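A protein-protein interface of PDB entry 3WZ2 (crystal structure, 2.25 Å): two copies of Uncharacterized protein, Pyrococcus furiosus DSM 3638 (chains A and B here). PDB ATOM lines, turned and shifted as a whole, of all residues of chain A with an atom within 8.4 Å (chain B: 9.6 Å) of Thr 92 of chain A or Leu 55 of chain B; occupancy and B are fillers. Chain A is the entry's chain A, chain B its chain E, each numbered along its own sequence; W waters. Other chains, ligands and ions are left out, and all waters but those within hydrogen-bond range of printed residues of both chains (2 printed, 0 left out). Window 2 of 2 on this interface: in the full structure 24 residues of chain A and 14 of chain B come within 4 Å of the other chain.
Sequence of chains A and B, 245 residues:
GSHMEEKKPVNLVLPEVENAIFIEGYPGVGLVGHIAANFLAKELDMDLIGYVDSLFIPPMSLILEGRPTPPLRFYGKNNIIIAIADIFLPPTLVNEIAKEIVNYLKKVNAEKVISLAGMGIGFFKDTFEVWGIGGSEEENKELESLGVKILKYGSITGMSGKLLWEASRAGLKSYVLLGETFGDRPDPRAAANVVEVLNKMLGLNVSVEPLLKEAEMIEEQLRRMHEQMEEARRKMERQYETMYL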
ATOM      1  N   PRO A   9      29.131  15.249  35.789  1.00  0.00           N
ATOM      2  CA  PRO A   9      28.879  14.815  34.400  1.00  0.00           C
ATOM      3  C   PRO A   9      29.999  15.142  33.399  1.00  0.00           C
ATOM      4  O   PRO A   9      30.258  14.349  32.491  1.00  0.00           O
ATOM      5  CB  PRO A   9      27.619  15.562  33.995  1.00  0.00           C
ATOM      6  CG  PRO A   9      27.581  16.749  34.881  1.00  0.00           C
ATOM      7  CD  PRO A   9      28.309  16.407  36.160  1.00  0.00           C
ATOM      8  N   VAL A  10      30.646  16.287  33.576  1.00  0.00           N
ATOM      9  CA  VAL A  10      31.862  16.603  32.850  1.00  0.00           C
ATOM     10  C   VAL A  10      32.929  17.052  33.822  1.00  0.00           C
ATOM     11  O   VAL A  10      32.670  17.935  34.632  1.00  0.00           O
ATOM     12  CB  VAL A  10      31.595  17.722  31.833  1.00  0.00           C
ATOM     13  CG1 VAL A  10      32.893  18.251  31.254  1.00  0.00           C
ATOM     14  CG2 VAL A  10      30.692  17.212  30.714  1.00  0.00           C
ATOM     15  N   PHE A  56      29.762  10.470  29.053  1.00  0.00           N
ATOM     16  CA  PHE A  56      28.922  10.655  27.881  1.00  0.00           C
ATOM     17  C   PHE A  56      29.718  10.879  26.609  1.00  0.00           C
ATOM     18  O   PHE A  56      29.152  10.938  25.528  1.00  0.00           O
ATOM     19  CB  PHE A  56      27.937  11.812  28.132  1.00  0.00           C
ATOM     20  CG  PHE A  56      27.041  11.578  29.315  1.00  0.00           C
ATOM     21  CD1 PHE A  56      27.328  12.155  30.546  1.00  0.00           C
ATOM     22  CD2 PHE A  56      25.928  10.732  29.208  1.00  0.00           C
ATOM     23  CE1 PHE A  56      26.504  11.939  31.642  1.00  0.00           C
ATOM     24  CE2 PHE A  56      25.109  10.484  30.307  1.00  0.00           C
ATOM     25  CZ  PHE A  56      25.397  11.100  31.522  1.00  0.00           C
ATOM     26  N   LEU A  89      29.506  16.714  19.311  1.00  0.00           N
ATOM     27  CA  LEU A  89      28.831  16.282  20.492  1.00  0.00           C
ATOM     28  C   LEU A  89      27.430  16.837  20.510  1.00  0.00           C
ATOM     29  O   LEU A  89      27.150  17.840  19.905  1.00  0.00           O
ATOM     30  CB  LEU A  89      29.610  16.747  21.720  1.00  0.00           C
ATOM     31  CG  LEU A  89      30.897  15.951  21.945  1.00  0.00           C
ATOM     32  CD1 LEU A  89      31.603  16.430  23.185  1.00  0.00           C
ATOM     33  CD2 LEU A  89      30.627  14.453  22.073  1.00  0.00           C
ATOM     34  N   PRO A  90      26.534  16.174  21.222  1.00  0.00           N
ATOM     35  CA  PRO A  90      25.206  16.736  21.371  1.00  0.00           C
ATOM     36  C   PRO A  90      25.125  18.023  22.205  1.00  0.00           C
ATOM     37  O   PRO A  90      25.997  18.288  23.048  1.00  0.00           O
ATOM     38  CB  PRO A  90      24.414  15.593  22.048  1.00  0.00           C
ATOM     39  CG  PRO A  90      25.431  14.756  22.715  1.00  0.00           C
ATOM     40  CD  PRO A  90      26.674  14.864  21.880  1.00  0.00           C
ATOM     41  N   PRO A  91      24.055  18.814  21.986  1.00  0.00           N
ATOM     42  CA  PRO A  91      23.949  20.176  22.467  1.00  0.00           C
ATOM     43  C   PRO A  91      24.080  20.322  23.978  1.00  0.00           C
ATOM     44  O   PRO A  91      24.776  21.242  24.465  1.00  0.00           O
ATOM     45  CB  PRO A  91      22.542  20.622  22.011  1.00  0.00           C
ATOM     46  CG  PRO A  91      21.887  19.427  21.398  1.00  0.00           C
ATOM     47  CD  PRO A  91      22.991  18.497  21.009  1.00  0.00           C
ATOM     48  N   THR A  92      23.391  19.467  24.720  1.00  0.00           N
ATOM     49  CA  THR A  92      23.450  19.566  26.171  1.00  0.00           C
ATOM     50  C   THR A  92      24.849  19.321  26.717  1.00  0.00           C
ATOM     51  O   THR A  92      25.286  19.977  27.640  1.00  0.00           O
ATOM     52  CB  THR A  92      22.451  18.587  26.817  1.00  0.00           C
ATOM     53  OG1 THR A  92      21.164  18.829  26.253  1.00  0.00           O
ATOM     54  CG2 THR A  92      22.366  18.820  28.300  1.00  0.00           C
ATOM     55  N   LEU A  93      25.561  18.394  26.102  1.00  0.00           N
ATOM     56  CA  LEU A  93      26.912  18.101  26.496  1.00  0.00           C
ATOM     57  C   LEU A  93      27.874  19.250  26.129  1.00  0.00           C
ATOM     58  O   LEU A  93      28.749  19.625  26.909  1.00  0.00           O
ATOM     59  CB  LEU A  93      27.345  16.791  25.865  1.00  0.00           C
ATOM     60  CG  LEU A  93      28.690  16.233  26.302  1.00  0.00           C
ATOM     61  CD1 LEU A  93      28.757  16.016  27.806  1.00  0.00           C
ATOM     62  CD2 LEU A  93      28.942  14.917  25.570  1.00  0.00           C
ATOM     63  N   VAL A  94      27.656  19.861  24.980  1.00  0.00           N
ATOM     64  CA  VAL A  94      28.392  21.085  24.614  1.00  0.00           C
ATOM     65  C   VAL A  94      28.176  22.144  25.668  1.00  0.00           C
ATOM     66  O   VAL A  94      29.138  22.772  26.094  1.00  0.00           O
ATOM     67  CB  VAL A  94      27.977  21.605  23.226  1.00  0.00           C
ATOM     68  CG1 VAL A  94      28.540  22.991  22.957  1.00  0.00           C
ATOM     69  CG2 VAL A  94      28.438  20.624  22.143  1.00  0.00           C
ATOM     70  N   ASN A  95      26.930  22.358  26.090  1.00  0.00           N
ATOM     71  CA  ASN A  95      26.683  23.355  27.153  1.00  0.00           C
ATOM     72  C   ASN A  95      27.378  23.013  28.449  1.00  0.00           C
ATOM     73  O   ASN A  95      27.915  23.885  29.085  1.00  0.00           O
ATOM     74  CB  ASN A  95      25.195  23.509  27.435  1.00  0.00           C
ATOM     75  CG  ASN A  95      24.476  24.241  26.337  1.00  0.00           C
ATOM     76  OD1 ASN A  95      25.035  25.155  25.696  1.00  0.00           O
ATOM     77  ND2 ASN A  95      23.213  23.886  26.129  1.00  0.00           N
ATOM     78  N   GLU A  96      27.362  21.737  28.850  1.00  0.00           N
ATOM     79  CA  GLU A  96      28.043  21.324  30.061  1.00  0.00           C
ATOM     80  C   GLU A  96      29.544  21.525  29.976  1.00  0.00           C
ATOM     81  O   GLU A  96      30.148  22.031  30.917  1.00  0.00           O
ATOM     82  CB  GLU A  96      27.774  19.874  30.385  1.00  0.00           C
ATOM     83  CG  GLU A  96      26.361  19.559  30.859  1.00  0.00           C
ATOM     84  CD  GLU A  96      26.180  19.728  32.369  1.00  0.00           C
ATOM     85  OE1 GLU A  96      27.004  20.447  33.023  1.00  0.00           O
ATOM     86  OE2 GLU A  96      25.216  19.112  32.908  1.00  0.00           O
ATOM     87  N   ILE A  97      30.136  21.217  28.825  1.00  0.00           N
ATOM     88  CA  ILE A  97      31.543  21.450  28.630  1.00  0.00           C
ATOM     89  C   ILE A  97      31.855  22.971  28.640  1.00  0.00           C
ATOM     90  O   ILE A  97      32.811  23.389  29.286  1.00  0.00           O
ATOM     91  CB  ILE A  97      32.066  20.795  27.332  1.00  0.00           C
ATOM     92  CG1 ILE A  97      31.962  19.281  27.438  1.00  0.00           C
ATOM     93  CG2 ILE A  97      33.506  21.195  27.070  1.00  0.00           C
ATOM     94  CD1 ILE A  97      31.969  18.577  26.114  1.00  0.00           C
ATOM     95  N   ALA A  98      31.071  23.779  27.922  1.00  0.00           N
ATOM     96  CA  ALA A  98      31.252  25.244  27.942  1.00  0.00           C
ATOM     97  C   ALA A  98      31.244  25.829  29.349  1.00  0.00           C
ATOM     98  O   ALA A  98      32.081  26.690  29.703  1.00  0.00           O
ATOM     99  CB  ALA A  98      30.218  25.940  27.094  1.00  0.00           C
ATOM    100  N   LYS A  99      30.300  25.359  30.141  1.00  0.00           N
ATOM    101  CA  LYS A  99      30.206  25.794  31.519  1.00  0.00           C
ATOM    102  C   LYS A  99      31.452  25.464  32.311  1.00  0.00           C
ATOM    103  O   LYS A  99      31.976  26.349  32.996  1.00  0.00           O
ATOM    104  CB  LYS A  99      28.961  25.210  32.182  1.00  0.00           C
ATOM    105  CG  LYS A  99      28.850  25.591  33.636  1.00  0.00           C
ATOM    106  CD  LYS A  99      27.675  24.994  34.378  1.00  0.00           C
ATOM    107  CE  LYS A  99      28.225  24.560  35.694  1.00  0.00           C
ATOM    108  NZ  LYS A  99      27.214  24.176  36.704  1.00  0.00           N
ATOM    109  N   GLU A 100      31.983  24.237  32.202  1.00  0.00           N
ATOM    110  CA  GLU A 100      33.245  23.928  32.863  1.00  0.00           C
ATOM    111  C   GLU A 100      34.420  24.729  32.297  1.00  0.00           C
ATOM    112  O   GLU A 100      35.311  25.150  33.032  1.00  0.00           O
ATOM    113  CB  GLU A 100      33.594  22.445  32.791  1.00  0.00           C
ATOM    114  CG  GLU A 100      32.626  21.523  33.514  1.00  0.00           C
ATOM    115  CD  GLU A 100      32.497  21.822  35.008  1.00  0.00           C
ATOM    116  OE1 GLU A 100      33.544  21.985  35.692  1.00  0.00           O
ATOM    117  OE2 GLU A 100      31.336  21.927  35.472  1.00  0.00           O
ATOM    118  N   LYS A 162      28.371  29.806  22.325  1.00  0.00           N
ATOM    119  CA  LYS A 162      28.142  29.722  23.749  1.00  0.00           C
ATOM    120  C   LYS A 162      29.251  30.352  24.521  1.00  0.00           C
ATOM    121  O   LYS A 162      29.004  31.144  25.414  1.00  0.00           O
ATOM    122  CB  LYS A 162      27.966  28.252  24.208  1.00  0.00           C
ATOM    123  CG  LYS A 162      27.388  28.101  25.599  1.00  0.00           C
ATOM    124  CD  LYS A 162      25.918  28.543  25.590  1.00  0.00           C
ATOM    125  CE  LYS A 162      25.354  28.815  26.971  1.00  0.00           C
ATOM    126  NZ  LYS A 162      25.150  27.551  27.706  1.00  0.00           N
ATOM    127  N   PRO B   9      17.367  23.742  36.788  1.00  0.00           N
ATOM    128  CA  PRO B   9      17.167  23.448  35.354  1.00  0.00           C
ATOM    129  C   PRO B   9      16.930  24.674  34.474  1.00  0.00           C
ATOM    130  O   PRO B   9      17.392  24.706  33.337  1.00  0.00           O
ATOM    131  CB  PRO B   9      15.917  22.574  35.329  1.00  0.00           C
ATOM    132  CG  PRO B   9      15.185  22.910  36.579  1.00  0.00           C
ATOM    133  CD  PRO B   9      16.195  23.372  37.603  1.00  0.00           C
ATOM    134  N   VAL B  10      16.214  25.663  35.004  1.00  0.00           N
ATOM    135  CA  VAL B  10      16.113  26.960  34.371  1.00  0.00           C
ATOM    136  C   VAL B  10      16.440  28.034  35.392  1.00  0.00           C
ATOM    137  O   VAL B  10      15.864  28.063  36.462  1.00  0.00           O
ATOM    138  CB  VAL B  10      14.696  27.185  33.838  1.00  0.00           C
ATOM    139  CG1 VAL B  10      14.490  28.618  33.407  1.00  0.00           C
ATOM    140  CG2 VAL B  10      14.452  26.262  32.667  1.00  0.00           C
ATOM    141  N   ASN B  11      17.292  28.976  35.017  1.00  0.00           N
ATOM    142  CA  ASN B  11      17.531  30.153  35.820  1.00  0.00           C
ATOM    143  C   ASN B  11      17.181  31.441  35.057  1.00  0.00           C
ATOM    144  O   ASN B  11      17.575  31.626  33.919  1.00  0.00           O
ATOM    145  CB  ASN B  11      19.003  30.089  36.210  1.00  0.00           C
ATOM    146  CG  ASN B  11      19.400  31.178  37.176  1.00  0.00           C
ATOM    147  OD1 ASN B  11      18.739  31.386  38.189  1.00  0.00           O
ATOM    148  ND2 ASN B  11      20.470  31.906  36.850  1.00  0.00           N
ATOM    149  N   TYR B  51      18.140  37.357  30.503  1.00  0.00           N
ATOM    150  CA  TYR B  51      17.990  36.193  29.657  1.00  0.00           C
ATOM    151  C   TYR B  51      17.555  34.990  30.469  1.00  0.00           C
ATOM    152  O   TYR B  51      17.600  35.011  31.694  1.00  0.00           O
ATOM    153  CB  TYR B  51      19.299  35.884  28.876  1.00  0.00           C
ATOM    154  CG  TYR B  51      20.550  35.312  29.625  1.00  0.00           C
ATOM    155  CD1 TYR B  51      21.288  36.078  30.502  1.00  0.00           C
ATOM    156  CD2 TYR B  51      20.994  33.992  29.393  1.00  0.00           C
ATOM    157  CE1 TYR B  51      22.401  35.549  31.145  1.00  0.00           C
ATOM    158  CE2 TYR B  51      22.123  33.450  30.002  1.00  0.00           C
ATOM    159  CZ  TYR B  51      22.822  34.230  30.889  1.00  0.00           C
ATOM    160  OH  TYR B  51      23.951  33.685  31.491  1.00  0.00           O
ATOM    161  N   VAL B  52      17.121  33.956  29.760  1.00  0.00           N
ATOM    162  CA  VAL B  52      16.917  32.657  30.355  1.00  0.00           C
ATOM    163  C   VAL B  52      18.137  31.790  30.127  1.00  0.00           C
ATOM    164  O   VAL B  52      18.648  31.709  29.033  1.00  0.00           O
ATOM    165  CB  VAL B  52      15.710  31.966  29.728  1.00  0.00           C
ATOM    166  CG1 VAL B  52      15.453  30.641  30.410  1.00  0.00           C
ATOM    167  CG2 VAL B  52      14.488  32.866  29.813  1.00  0.00           C
ATOM    168  N   ASP B  53      18.576  31.135  31.181  1.00  0.00           N
ATOM    169  CA  ASP B  53      19.779  30.348  31.160  1.00  0.00           C
ATOM    170  C   ASP B  53      19.430  28.915  31.553  1.00  0.00           C
ATOM    171  O   ASP B  53      18.861  28.676  32.618  1.00  0.00           O
ATOM    172  CB  ASP B  53      20.782  30.934  32.142  1.00  0.00           C
ATOM    173  CG  ASP B  53      22.080  30.184  32.166  1.00  0.00           C
ATOM    174  OD1 ASP B  53      22.515  29.659  31.100  1.00  0.00           O
ATOM    175  OD2 ASP B  53      22.674  30.114  33.270  1.00  0.00           O
ATOM    176  N   SER B  54      19.774  27.970  30.691  1.00  0.00           N
ATOM    177  CA  SER B  54      19.505  26.574  30.917  1.00  0.00           C
ATOM    178  C   SER B  54      20.403  25.725  30.025  1.00  0.00           C
ATOM    179  O   SER B  54      20.571  26.010  28.845  1.00  0.00           O
ATOM    180  CB  SER B  54      18.039  26.284  30.570  1.00  0.00           C
ATOM    181  OG  SER B  54      17.727  24.915  30.655  1.00  0.00           O
ATOM    182  N   LEU B  55      20.892  24.629  30.579  1.00  0.00           N
ATOM    183  CA  LEU B  55      21.593  23.628  29.818  1.00  0.00           C
ATOM    184  C   LEU B  55      20.761  23.043  28.715  1.00  0.00           C
ATOM    185  O   LEU B  55      21.311  22.421  27.821  1.00  0.00           O
ATOM    186  CB  LEU B  55      22.063  22.472  30.723  1.00  0.00           C
ATOM    187  CG  LEU B  55      23.021  22.867  31.846  1.00  0.00           C
ATOM    188  CD1 LEU B  55      23.166  21.697  32.815  1.00  0.00           C
ATOM    189  CD2 LEU B  55      24.373  23.313  31.297  1.00  0.00           C
ATOM    190  N   PHE B  56      19.443  23.191  28.781  1.00  0.00           N
ATOM    191  CA  PHE B  56      18.588  22.567  27.774  1.00  0.00           C
ATOM    192  C   PHE B  56      18.258  23.487  26.602  1.00  0.00           C
ATOM    193  O   PHE B  56      17.609  23.077  25.658  1.00  0.00           O
ATOM    194  CB  PHE B  56      17.327  22.016  28.467  1.00  0.00           C
ATOM    195  CG  PHE B  56      17.644  21.023  29.556  1.00  0.00           C
ATOM    196  CD1 PHE B  56      18.004  19.713  29.241  1.00  0.00           C
ATOM    197  CD2 PHE B  56      17.651  21.410  30.890  1.00  0.00           C
ATOM    198  CE1 PHE B  56      18.346  18.810  30.237  1.00  0.00           C
ATOM    199  CE2 PHE B  56      17.973  20.503  31.899  1.00  0.00           C
ATOM    200  CZ  PHE B  56      18.331  19.208  31.567  1.00  0.00           C
ATOM    201  N   ILE B  57      18.704  24.739  26.681  1.00  0.00           N
ATOM    202  CA  ILE B  57      18.673  25.633  25.545  1.00  0.00           C
ATOM    203  C   ILE B  57      19.928  25.379  24.678  1.00  0.00           C
ATOM    204  O   ILE B  57      21.038  25.352  25.202  1.00  0.00           O
ATOM    205  CB  ILE B  57      18.647  27.101  26.014  1.00  0.00           C
ATOM    206  CG1 ILE B  57      17.307  27.399  26.689  1.00  0.00           C
ATOM    207  CG2 ILE B  57      18.860  28.032  24.825  1.00  0.00           C
ATOM    208  CD1 ILE B  57      17.309  28.683  27.480  1.00  0.00           C
ATOM    209  N   PRO B  58      19.748  25.132  23.373  1.00  0.00           N
ATOM    210  CA  PRO B  58      20.928  24.694  22.635  1.00  0.00           C
ATOM    211  C   PRO B  58      21.946  25.832  22.479  1.00  0.00           C
ATOM    212  O   PRO B  58      21.570  26.986  22.549  1.00  0.00           O
ATOM    213  CB  PRO B  58      20.381  24.232  21.273  1.00  0.00           C
ATOM    214  CG  PRO B  58      18.932  24.565  21.258  1.00  0.00           C
ATOM    215  CD  PRO B  58      18.492  24.911  22.646  1.00  0.00           C
ATOM    216  N   PRO B  59      23.223  25.487  22.344  1.00  0.00           N
ATOM    217  CA  PRO B  59      24.325  26.465  22.440  1.00  0.00           C
ATOM    218  C   PRO B  59      24.340  27.363  21.231  1.00  0.00           C
ATOM    219  O   PRO B  59      24.341  26.863  20.107  1.00  0.00           O
ATOM    220  CB  PRO B  59      25.578  25.593  22.465  1.00  0.00           C
ATOM    221  CG  PRO B  59      25.155  24.264  21.901  1.00  0.00           C
ATOM    222  CD  PRO B  59      23.711  24.102  22.223  1.00  0.00           C
ATOM    223  N   MET B  60      24.338  28.669  21.460  1.00  0.00           N
ATOM    224  CA  MET B  60      24.368  29.669  20.379  1.00  0.00           C
ATOM    225  C   MET B  60      24.458  31.059  20.967  1.00  0.00           C
ATOM    226  O   MET B  60      24.056  31.262  22.104  1.00  0.00           O
ATOM    227  CB  MET B  60      23.136  29.608  19.495  1.00  0.00           C
ATOM    228  CG  MET B  60      21.890  30.056  20.184  1.00  0.00           C
ATOM    229  SD  MET B  60      20.450  29.720  19.154  1.00  0.00           S
ATOM    230  CE  MET B  60      20.960  30.371  17.578  1.00  0.00           C
ATOM    231  N   LEU B  89      10.629  25.803  21.870  1.00  0.00           N
ATOM    232  CA  LEU B  89      11.151  24.934  22.883  1.00  0.00           C
ATOM    233  C   LEU B  89      10.177  23.798  23.179  1.00  0.00           C
ATOM    234  O   LEU B  89       8.994  23.915  22.932  1.00  0.00           O
ATOM    235  CB  LEU B  89      11.422  25.749  24.138  1.00  0.00           C
ATOM    236  CG  LEU B  89      12.641  26.680  23.996  1.00  0.00           C
ATOM    237  CD1 LEU B  89      12.879  27.414  25.279  1.00  0.00           C
ATOM    238  CD2 LEU B  89      13.905  25.896  23.621  1.00  0.00           C
ATOM    239  N   PRO B  90      10.681  22.684  23.694  1.00  0.00           N
ATOM    240  CA  PRO B  90       9.789  21.603  24.073  1.00  0.00           C
ATOM    241  C   PRO B  90       8.915  21.916  25.294  1.00  0.00           C
ATOM    242  O   PRO B  90       9.259  22.785  26.103  1.00  0.00           O
ATOM    243  CB  PRO B  90      10.742  20.439  24.370  1.00  0.00           C
ATOM    244  CG  PRO B  90      12.061  21.071  24.657  1.00  0.00           C
ATOM    245  CD  PRO B  90      12.102  22.324  23.834  1.00  0.00           C
ATOM    246  N   LEU B  93      10.020  22.253  29.017  1.00  0.00           N
ATOM    247  CA  LEU B  93      10.900  23.384  29.237  1.00  0.00           C
ATOM    248  C   LEU B  93      10.099  24.688  29.234  1.00  0.00           C
ATOM    249  O   LEU B  93      10.357  25.574  30.045  1.00  0.00           O
ATOM    250  CB  LEU B  93      11.993  23.384  28.176  1.00  0.00           C
ATOM    251  CG  LEU B  93      13.106  24.425  28.314  1.00  0.00           C
ATOM    252  CD1 LEU B  93      13.818  24.282  29.642  1.00  0.00           C
ATOM    253  CD2 LEU B  93      14.096  24.245  27.167  1.00  0.00           C
HETATM  254  O   HOH W   1      20.650  21.500  24.774  1.00  0.00           O
HETATM  255  O   HOH W   2      22.399  27.394  26.640  1.00  0.00           O
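The side-chain amide nitrogen (ND2) of Asn 95 of chain A sits at hydrogen-bond distance from the backbone carbonyl oxygen (O) of Leu 55 of chain B, at 2.9 Å.
The side-chain amide nitrogen (ND2) of Asn 95 of chain A sits at hydrogen-bond distance from the backbone carbonyl oxygen (O) of Ile 57 of chain B (2.8 Å).
The side-chain amide oxygen (OD1) of Asn 95 of chain A lies within hydrogen-bond range of the side-chain amino group (NZ) of Lys 162 of chain A (3.1 Å).
The backbone carbonyl oxygen (O) of Pro 91 of chain A lies within hydrogen-bond range of the side-chain amide nitrogen (ND2) of Asn 95 of chain A (3.5 Å).
Among the printed residues, pairs that only touch across the chains: Pro 91 of chain A with Pro 59 of chain B (3.7 Å), Thr 92 of chain A with Leu 55 of chain B (3.8 Å), Val 94 of chain A with Pro 59 of chain B (3.8 Å), Asn 95 of chain A with Pro 59 of chain B (3.3 Å), Glu 96 of chain A with Leu 55 of chain B (3.3 Å) and Lys 162 of chain A with Pro 59 of chain B (3.98 Å).
Of chain B, only Pro 59 (3.7 Å) comes within 4 Å of Pro 91 of chain A.
Of the printed residues of chain B, Thr 92 of chain A touches Leu 55.
Printed residues of chain B within 4 Å of Val 94 of chain A: Pro 59 (3.8 Å).
Of the printed residues of chain B, Glu 96 of chain A touches Leu 55 (3.3 Å).
No residue of chain A comes within 4 Å of Ser 54 of chain B.
Of chain A, only Thr 92 (3.8 Å), Asn 95 (2.9 Å) and Glu 96 (3.3 Å) come within 4 Å of Leu 55 of chain B.
Of the printed residues of chain A, Ile 57 of chain B touches Asn 95.
Of the printed residues of chain A, Pro 59 of chain B touches Pro 91 (3.7 Å), Val 94 (3.8 Å), Asn 95 (3.3 Å) and Lys 162 (3.98 Å).
Printed residues of chain B that touch a printed residue of chain A: Leu 55, Ile 57 and Pro 59.
Hydrophobic or aromatic side chains of chain B that line the printed part of chain A: Leu 55 and Pro 59.
Along chain B the printed residues that touch a printed residue of chain A span positions 55 to 59.
Among the printed residues, 8 pairs touch across the chains.
Among the printed residues, no Asp or Glu carboxylate lies within 4 Å of a Lys or Arg side-chain nitrogen of the other chain.
6 positions are printed for both chains.
Of the 8 pairs that touch across the chains among the printed residues, none has its exchanged pair printed and touching as well.
Water W2 lies within hydrogen-bond range of O of Ile 57 of chain B (2.8 Å), NZ of Lys 162 of chain A (3.0 Å) and O of Ser 54 of chain B (3.2 Å).
Water W1 bridges the side-chain hydroxyl (OG1) of Thr 92 of chain A and the backbone carbonyl oxygen (O) of Leu 55 of chain B.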
